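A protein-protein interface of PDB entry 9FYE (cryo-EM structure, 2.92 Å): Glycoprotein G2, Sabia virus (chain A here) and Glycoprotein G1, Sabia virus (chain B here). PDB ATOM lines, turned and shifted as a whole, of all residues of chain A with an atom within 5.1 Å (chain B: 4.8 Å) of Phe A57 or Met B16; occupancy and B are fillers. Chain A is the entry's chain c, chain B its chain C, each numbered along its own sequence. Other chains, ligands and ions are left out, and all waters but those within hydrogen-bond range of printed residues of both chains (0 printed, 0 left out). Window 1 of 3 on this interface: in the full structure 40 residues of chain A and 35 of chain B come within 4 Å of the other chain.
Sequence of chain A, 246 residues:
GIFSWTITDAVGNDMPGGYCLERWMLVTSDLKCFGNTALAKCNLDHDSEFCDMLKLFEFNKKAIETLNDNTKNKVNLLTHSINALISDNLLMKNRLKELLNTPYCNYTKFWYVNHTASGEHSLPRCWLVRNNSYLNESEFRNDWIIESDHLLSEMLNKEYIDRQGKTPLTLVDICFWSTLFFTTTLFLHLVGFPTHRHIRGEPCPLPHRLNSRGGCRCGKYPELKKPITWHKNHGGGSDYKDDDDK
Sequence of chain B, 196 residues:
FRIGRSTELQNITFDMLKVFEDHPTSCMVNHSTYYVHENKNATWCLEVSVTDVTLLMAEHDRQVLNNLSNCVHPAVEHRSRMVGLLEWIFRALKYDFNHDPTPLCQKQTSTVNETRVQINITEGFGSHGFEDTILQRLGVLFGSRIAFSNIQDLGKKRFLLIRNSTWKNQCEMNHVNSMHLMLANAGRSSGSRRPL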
ATOM      1  N   TYR A  19      11.692  12.879  12.623  1.00  0.00           N
ATOM      2  CA  TYR A  19      12.625  11.876  12.119  1.00  0.00           C
ATOM      3  C   TYR A  19      11.838  10.634  11.720  1.00  0.00           C
ATOM      4  O   TYR A  19      11.279   9.947  12.577  1.00  0.00           O
ATOM      5  CB  TYR A  19      13.679  11.546  13.170  1.00  0.00           C
ATOM      6  CG  TYR A  19      14.716  10.550  12.705  1.00  0.00           C
ATOM      7  CD1 TYR A  19      15.745  10.933  11.858  1.00  0.00           C
ATOM      8  CD2 TYR A  19      14.667   9.227  13.118  1.00  0.00           C
ATOM      9  CE1 TYR A  19      16.694  10.024  11.432  1.00  0.00           C
ATOM     10  CE2 TYR A  19      15.610   8.313  12.700  1.00  0.00           C
ATOM     11  CZ  TYR A  19      16.621   8.715  11.857  1.00  0.00           C
ATOM     12  OH  TYR A  19      17.563   7.805  11.438  1.00  0.00           O
ATOM     13  N   LEU A  21      11.717   6.911  10.325  1.00  0.00           N
ATOM     14  CA  LEU A  21      12.528   5.715  10.155  1.00  0.00           C
ATOM     15  C   LEU A  21      12.190   5.031   8.837  1.00  0.00           C
ATOM     16  O   LEU A  21      11.031   4.999   8.416  1.00  0.00           O
ATOM     17  CB  LEU A  21      12.306   4.745  11.315  1.00  0.00           C
ATOM     18  CG  LEU A  21      12.923   5.096  12.668  1.00  0.00           C
ATOM     19  CD1 LEU A  21      12.282   4.257  13.753  1.00  0.00           C
ATOM     20  CD2 LEU A  21      14.422   4.897  12.661  1.00  0.00           C
ATOM     21  N   TRP A  24      13.394  -0.473   5.867  1.00  0.00           N
ATOM     22  CA  TRP A  24      14.302  -1.562   6.202  1.00  0.00           C
ATOM     23  C   TRP A  24      14.724  -1.524   7.666  1.00  0.00           C
ATOM     24  O   TRP A  24      15.098  -2.561   8.225  1.00  0.00           O
ATOM     25  CB  TRP A  24      15.515  -1.536   5.270  1.00  0.00           C
ATOM     26  CG  TRP A  24      16.381  -0.321   5.391  1.00  0.00           C
ATOM     27  CD1 TRP A  24      16.283   0.826   4.662  1.00  0.00           C
ATOM     28  CD2 TRP A  24      17.499  -0.145   6.267  1.00  0.00           C
ATOM     29  NE1 TRP A  24      17.260   1.713   5.041  1.00  0.00           N
ATOM     30  CE2 TRP A  24      18.021   1.139   6.025  1.00  0.00           C
ATOM     31  CE3 TRP A  24      18.104  -0.945   7.239  1.00  0.00           C
ATOM     32  CZ2 TRP A  24      19.116   1.642   6.719  1.00  0.00           C
ATOM     33  CZ3 TRP A  24      19.193  -0.444   7.925  1.00  0.00           C
ATOM     34  CH2 TRP A  24      19.687   0.836   7.663  1.00  0.00           C
ATOM     35  N   MET A  25      14.695  -0.346   8.294  1.00  0.00           N
ATOM     36  CA  MET A  25      15.106  -0.240   9.689  1.00  0.00           C
ATOM     37  C   MET A  25      14.199  -1.049  10.608  1.00  0.00           C
ATOM     38  O   MET A  25      14.679  -1.736  11.516  1.00  0.00           O
ATOM     39  CB  MET A  25      15.134   1.226  10.118  1.00  0.00           C
ATOM     40  CG  MET A  25      16.116   2.078   9.339  1.00  0.00           C
ATOM     41  SD  MET A  25      15.884   3.839   9.619  1.00  0.00           S
ATOM     42  CE  MET A  25      17.416   4.489   8.970  1.00  0.00           C
ATOM     43  N   MET A  53      20.754   3.346  19.099  1.00  0.00           N
ATOM     44  CA  MET A  53      20.347   2.665  17.876  1.00  0.00           C
ATOM     45  C   MET A  53      20.040   3.660  16.766  1.00  0.00           C
ATOM     46  O   MET A  53      20.363   3.419  15.597  1.00  0.00           O
ATOM     47  CB  MET A  53      19.143   1.770  18.154  1.00  0.00           C
ATOM     48  CG  MET A  53      19.416   0.645  19.142  1.00  0.00           C
ATOM     49  SD  MET A  53      20.630  -0.557  18.574  1.00  0.00           S
ATOM     50  CE  MET A  53      22.091   0.002  19.435  1.00  0.00           C
ATOM     51  N   LEU A  54      19.410   4.785  17.109  1.00  0.00           N
ATOM     52  CA  LEU A  54      19.184   5.822  16.108  1.00  0.00           C
ATOM     53  C   LEU A  54      20.496   6.409  15.607  1.00  0.00           C
ATOM     54  O   LEU A  54      20.619   6.749  14.427  1.00  0.00           O
ATOM     55  CB  LEU A  54      18.294   6.921  16.670  1.00  0.00           C
ATOM     56  CG  LEU A  54      16.856   6.516  16.948  1.00  0.00           C
ATOM     57  CD1 LEU A  54      16.154   7.702  17.512  1.00  0.00           C
ATOM     58  CD2 LEU A  54      16.167   6.037  15.689  1.00  0.00           C
ATOM     59  N   LYS A  55      21.478   6.568  16.496  1.00  0.00           N
ATOM     60  CA  LYS A  55      22.787   7.050  16.065  1.00  0.00           C
ATOM     61  C   LYS A  55      23.442   6.070  15.102  1.00  0.00           C
ATOM     62  O   LYS A  55      24.068   6.478  14.117  1.00  0.00           O
ATOM     63  CB  LYS A  55      23.685   7.296  17.276  1.00  0.00           C
ATOM     64  CG  LYS A  55      23.430   8.620  17.968  1.00  0.00           C
ATOM     65  CD  LYS A  55      24.598   9.014  18.855  1.00  0.00           C
ATOM     66  CE  LYS A  55      24.580   8.280  20.181  1.00  0.00           C
ATOM     67  NZ  LYS A  55      23.507   8.799  21.070  1.00  0.00           N
ATOM     68  N   LEU A  56      23.299   4.772  15.368  1.00  0.00           N
ATOM     69  CA  LEU A  56      23.796   3.762  14.438  1.00  0.00           C
ATOM     70  C   LEU A  56      23.095   3.854  13.090  1.00  0.00           C
ATOM     71  O   LEU A  56      23.736   3.745  12.039  1.00  0.00           O
ATOM     72  CB  LEU A  56      23.617   2.369  15.036  1.00  0.00           C
ATOM     73  CG  LEU A  56      24.832   1.799  15.757  1.00  0.00           C
ATOM     74  CD1 LEU A  56      25.180   2.661  16.935  1.00  0.00           C
ATOM     75  CD2 LEU A  56      24.531   0.395  16.219  1.00  0.00           C
ATOM     76  N   PHE A  57      21.775   4.041  13.099  1.00  0.00           N
ATOM     77  CA  PHE A  57      21.040   4.187  11.846  1.00  0.00           C
ATOM     78  C   PHE A  57      21.488   5.421  11.071  1.00  0.00           C
ATOM     79  O   PHE A  57      21.645   5.370   9.846  1.00  0.00           O
ATOM     80  CB  PHE A  57      19.540   4.241  12.120  1.00  0.00           C
ATOM     81  CG  PHE A  57      18.907   2.892  12.283  1.00  0.00           C
ATOM     82  CD1 PHE A  57      19.262   1.843  11.455  1.00  0.00           C
ATOM     83  CD2 PHE A  57      17.946   2.676  13.252  1.00  0.00           C
ATOM     84  CE1 PHE A  57      18.678   0.603  11.596  1.00  0.00           C
ATOM     85  CE2 PHE A  57      17.361   1.439  13.395  1.00  0.00           C
ATOM     86  CZ  PHE A  57      17.728   0.401  12.565  1.00  0.00           C
ATOM     87  N   GLU A  58      21.690   6.543  11.766  1.00  0.00           N
ATOM     88  CA  GLU A  58      22.143   7.761  11.098  1.00  0.00           C
ATOM     89  C   GLU A  58      23.535   7.577  10.512  1.00  0.00           C
ATOM     90  O   GLU A  58      23.810   8.018   9.388  1.00  0.00           O
ATOM     91  CB  GLU A  58      22.133   8.936  12.075  1.00  0.00           C
ATOM     92  CG  GLU A  58      20.751   9.351  12.549  1.00  0.00           C
ATOM     93  CD  GLU A  58      20.787  10.087  13.877  1.00  0.00           C
ATOM     94  OE1 GLU A  58      21.898  10.360  14.377  1.00  0.00           O
ATOM     95  OE2 GLU A  58      19.705  10.388  14.423  1.00  0.00           O
ATOM     96  N   PHE A  59      24.430   6.934  11.264  1.00  0.00           N
ATOM     97  CA  PHE A  59      25.766   6.660  10.750  1.00  0.00           C
ATOM     98  C   PHE A  59      25.706   5.766   9.520  1.00  0.00           C
ATOM     99  O   PHE A  59      26.425   5.997   8.542  1.00  0.00           O
ATOM    100  CB  PHE A  59      26.623   6.026  11.845  1.00  0.00           C
ATOM    101  CG  PHE A  59      27.970   5.564  11.373  1.00  0.00           C
ATOM    102  CD1 PHE A  59      28.144   4.295  10.846  1.00  0.00           C
ATOM    103  CD2 PHE A  59      29.063   6.406  11.450  1.00  0.00           C
ATOM    104  CE1 PHE A  59      29.380   3.878  10.410  1.00  0.00           C
ATOM    105  CE2 PHE A  59      30.300   5.990  11.017  1.00  0.00           C
ATOM    106  CZ  PHE A  59      30.458   4.726  10.497  1.00  0.00           C
ATOM    107  N   ASN A  60      24.860   4.735   9.551  1.00  0.00           N
ATOM    108  CA  ASN A  60      24.739   3.846   8.401  1.00  0.00           C
ATOM    109  C   ASN A  60      24.198   4.591   7.189  1.00  0.00           C
ATOM    110  O   ASN A  60      24.659   4.378   6.062  1.00  0.00           O
ATOM    111  CB  ASN A  60      23.842   2.660   8.750  1.00  0.00           C
ATOM    112  CG  ASN A  60      23.878   1.572   7.701  1.00  0.00           C
ATOM    113  OD1 ASN A  60      22.867   1.268   7.072  1.00  0.00           O
ATOM    114  ND2 ASN A  60      25.046   0.970   7.513  1.00  0.00           N
ATOM    115  N   LYS A  61      23.224   5.477   7.403  1.00  0.00           N
ATOM    116  CA  LYS A  61      22.671   6.253   6.298  1.00  0.00           C
ATOM    117  C   LYS A  61      23.729   7.161   5.683  1.00  0.00           C
ATOM    118  O   LYS A  61      23.874   7.226   4.456  1.00  0.00           O
ATOM    119  CB  LYS A  61      21.475   7.070   6.784  1.00  0.00           C
ATOM    120  CG  LYS A  61      20.789   7.877   5.701  1.00  0.00           C
ATOM    121  CD  LYS A  61      19.530   8.537   6.229  1.00  0.00           C
ATOM    122  CE  LYS A  61      19.865   9.691   7.157  1.00  0.00           C
ATOM    123  NZ  LYS A  61      18.651  10.454   7.556  1.00  0.00           N
ATOM    124  N   LYS A  62      24.489   7.865   6.527  1.00  0.00           N
ATOM    125  CA  LYS A  62      25.537   8.742   6.011  1.00  0.00           C
ATOM    126  C   LYS A  62      26.627   7.944   5.301  1.00  0.00           C
ATOM    127  O   LYS A  62      27.175   8.396   4.289  1.00  0.00           O
ATOM    128  CB  LYS A  62      26.112   9.605   7.139  1.00  0.00           C
ATOM    129  CG  LYS A  62      27.375   9.084   7.801  1.00  0.00           C
ATOM    130  CD  LYS A  62      28.010  10.155   8.672  1.00  0.00           C
ATOM    131  CE  LYS A  62      29.142   9.585   9.505  1.00  0.00           C
ATOM    132  NZ  LYS A  62      30.163   8.911   8.659  1.00  0.00           N
ATOM    133  N   TYR A 107      18.141  -4.603  22.905  1.00  0.00           N
ATOM    134  CA  TYR A 107      18.295  -3.639  21.813  1.00  0.00           C
ATOM    135  C   TYR A 107      17.460  -3.985  20.586  1.00  0.00           C
ATOM    136  O   TYR A 107      17.791  -3.574  19.473  1.00  0.00           O
ATOM    137  CB  TYR A 107      19.764  -3.485  21.416  1.00  0.00           C
ATOM    138  CG  TYR A 107      20.624  -2.830  22.466  1.00  0.00           C
ATOM    139  CD1 TYR A 107      21.209  -3.577  23.474  1.00  0.00           C
ATOM    140  CD2 TYR A 107      20.861  -1.467  22.444  1.00  0.00           C
ATOM    141  CE1 TYR A 107      21.990  -2.986  24.437  1.00  0.00           C
ATOM    142  CE2 TYR A 107      21.649  -0.867  23.396  1.00  0.00           C
ATOM    143  CZ  TYR A 107      22.211  -1.631  24.392  1.00  0.00           C
ATOM    144  OH  TYR A 107      22.996  -1.035  25.346  1.00  0.00           O
ATOM    145  N   PHE B  14      13.221  -3.372  16.062  1.00  0.00           N
ATOM    146  CA  PHE B  14      14.340  -2.941  15.235  1.00  0.00           C
ATOM    147  C   PHE B  14      14.887  -4.102  14.421  1.00  0.00           C
ATOM    148  O   PHE B  14      15.094  -5.199  14.950  1.00  0.00           O
ATOM    149  CB  PHE B  14      15.462  -2.353  16.096  1.00  0.00           C
ATOM    150  CG  PHE B  14      15.298  -0.896  16.413  1.00  0.00           C
ATOM    151  CD1 PHE B  14      14.437  -0.104  15.683  1.00  0.00           C
ATOM    152  CD2 PHE B  14      16.013  -0.316  17.445  1.00  0.00           C
ATOM    153  CE1 PHE B  14      14.298   1.240  15.970  1.00  0.00           C
ATOM    154  CE2 PHE B  14      15.873   1.023  17.736  1.00  0.00           C
ATOM    155  CZ  PHE B  14      15.019   1.802  16.995  1.00  0.00           C
ATOM    156  N   ASP B  15      15.116  -3.854  13.136  1.00  0.00           N
ATOM    157  CA  ASP B  15      15.818  -4.775  12.252  1.00  0.00           C
ATOM    158  C   ASP B  15      17.207  -4.194  12.023  1.00  0.00           C
ATOM    159  O   ASP B  15      17.355  -3.187  11.324  1.00  0.00           O
ATOM    160  CB  ASP B  15      15.060  -4.955  10.939  1.00  0.00           C
ATOM    161  CG  ASP B  15      15.555  -6.136  10.133  1.00  0.00           C
ATOM    162  OD1 ASP B  15      16.606  -6.708  10.486  1.00  0.00           O
ATOM    163  OD2 ASP B  15      14.892  -6.491   9.136  1.00  0.00           O
ATOM    164  N   MET B  16      18.223  -4.819  12.620  1.00  0.00           N
ATOM    165  CA  MET B  16      19.596  -4.336  12.544  1.00  0.00           C
ATOM    166  C   MET B  16      20.480  -5.217  11.674  1.00  0.00           C
ATOM    167  O   MET B  16      21.708  -5.116  11.745  1.00  0.00           O
ATOM    168  CB  MET B  16      20.195  -4.218  13.942  1.00  0.00           C
ATOM    169  CG  MET B  16      19.450  -3.275  14.844  1.00  0.00           C
ATOM    170  SD  MET B  16      19.988  -1.583  14.584  1.00  0.00           S
ATOM    171  CE  MET B  16      18.836  -0.740  15.639  1.00  0.00           C
ATOM    172  N   LEU B  17      19.882  -6.089  10.862  1.00  0.00           N
ATOM    173  CA  LEU B  17      20.677  -6.974  10.020  1.00  0.00           C
ATOM    174  C   LEU B  17      21.510  -6.184   9.020  1.00  0.00           C
ATOM    175  O   LEU B  17      22.709  -6.432   8.861  1.00  0.00           O
ATOM    176  CB  LEU B  17      19.762  -7.959   9.294  1.00  0.00           C
ATOM    177  CG  LEU B  17      20.396  -8.737   8.142  1.00  0.00           C
ATOM    178  CD1 LEU B  17      21.496  -9.649   8.658  1.00  0.00           C
ATOM    179  CD2 LEU B  17      19.345  -9.529   7.385  1.00  0.00           C
ATOM    180  N   LYS B  18      20.892  -5.211   8.350  1.00  0.00           N
ATOM    181  CA  LYS B  18      21.588  -4.479   7.294  1.00  0.00           C
ATOM    182  C   LYS B  18      22.711  -3.614   7.854  1.00  0.00           C
ATOM    183  O   LYS B  18      23.758  -3.461   7.216  1.00  0.00           O
ATOM    184  CB  LYS B  18      20.588  -3.639   6.503  1.00  0.00           C
ATOM    185  CG  LYS B  18      21.182  -2.962   5.288  1.00  0.00           C
ATOM    186  CD  LYS B  18      20.118  -2.225   4.501  1.00  0.00           C
ATOM    187  CE  LYS B  18      20.709  -1.599   3.257  1.00  0.00           C
ATOM    188  NZ  LYS B  18      21.678  -0.538   3.620  1.00  0.00           N
ATOM    189  N   VAL B  19      22.510  -3.029   9.037  1.00  0.00           N
ATOM    190  CA  VAL B  19      23.559  -2.220   9.654  1.00  0.00           C
ATOM    191  C   VAL B  19      24.768  -3.079  10.000  1.00  0.00           C
ATOM    192  O   VAL B  19      25.918  -2.657   9.835  1.00  0.00           O
ATOM    193  CB  VAL B  19      23.012  -1.491  10.896  1.00  0.00           C
ATOM    194  CG1 VAL B  19      24.108  -0.684  11.569  1.00  0.00           C
ATOM    195  CG2 VAL B  19      21.851  -0.596  10.521  1.00  0.00           C
ATOM    196  N   PHE B  20      24.529  -4.300  10.478  1.00  0.00           N
ATOM    197  CA  PHE B  20      25.574  -5.160  11.018  1.00  0.00           C
ATOM    198  C   PHE B  20      25.964  -6.300  10.082  1.00  0.00           C
ATOM    199  O   PHE B  20      26.705  -7.195  10.496  1.00  0.00           O
ATOM    200  CB  PHE B  20      25.114  -5.738  12.358  1.00  0.00           C
ATOM    201  CG  PHE B  20      25.098  -4.747  13.483  1.00  0.00           C
ATOM    202  CD1 PHE B  20      26.252  -4.452  14.176  1.00  0.00           C
ATOM    203  CD2 PHE B  20      23.926  -4.122  13.855  1.00  0.00           C
ATOM    204  CE1 PHE B  20      26.243  -3.552  15.211  1.00  0.00           C
ATOM    205  CE2 PHE B  20      23.912  -3.218  14.890  1.00  0.00           C
ATOM    206  CZ  PHE B  20      25.075  -2.935  15.568  1.00  0.00           C
ATOM    207  N   HIS B 175      23.098  -8.991  17.004  1.00  0.00           N
ATOM    208  CA  HIS B 175      23.803  -7.724  16.842  1.00  0.00           C
ATOM    209  C   HIS B 175      24.335  -7.156  18.152  1.00  0.00           C
ATOM    210  O   HIS B 175      25.122  -6.205  18.122  1.00  0.00           O
ATOM    211  CB  HIS B 175      22.909  -6.702  16.128  1.00  0.00           C
ATOM    212  CG  HIS B 175      21.748  -6.215  16.938  1.00  0.00           C
ATOM    213  ND1 HIS B 175      21.762  -5.013  17.611  1.00  0.00           N
ATOM    214  CD2 HIS B 175      20.522  -6.748  17.149  1.00  0.00           C
ATOM    215  CE1 HIS B 175      20.605  -4.838  18.222  1.00  0.00           C
ATOM    216  NE2 HIS B 175      19.835  -5.877  17.959  1.00  0.00           N
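OD1 of Asp B15 sits at hydrogen-bond distance from N of Leu B17 (3.4 Å).
Trp A24 touches Asp B15. CD of Lys B18 touches CE3 of Trp A24, 3.6 Å away. CZ3 of Trp A24 touches CG2 of Val B19 (3.7 Å). Met A25 touches Phe B14 (O to C, 3.8 Å). CB of Met A53 touches CE2 of Phe B14, at 3.4 Å. CE of Met B16 touches SD of Met A53, at 3.4 Å. Leu A56 touches Phe B20 (CD2 to CZ, 3.4 Å). Asp B15 touches Phe A57. Phe A57 touches Met B16. Phe A57 touches Val B19.
Of the printed residues of chain B, Phe A57 touches Asp B15, Met B16 and Val B19. Printed residues of chain B within 4 Å of Leu A56: Phe B20 (3.4 Å). Of the printed residues of chain B, Met A53 touches Phe B14 (3.4 Å) and Met B16 (3.4 Å). Printed residues of chain B within 4 Å of Met A25: Phe B14 and Asp B15. Of the printed residues of chain B, Tyr A107 touches His B175. Leu B17 touches none of the printed residues of chain A. Lys A61 touches none of the printed residues of chain B. The nearest printed residue of chain A that does not touch Lys B18 is Asn A60 (4.1 Å).
The backbone carbonyl oxygen of Tyr A107 lies close to a ring nitrogen (NE2) of His B175 (3.4 Å). The backbone NH (N) of Asp B15 is in hydrogen-bond range of the backbone carbonyl oxygen (O) of Met A25, 2.7 Å away.
Along chain B the printed residues that touch a printed residue of chain A span positions 14 to 175.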
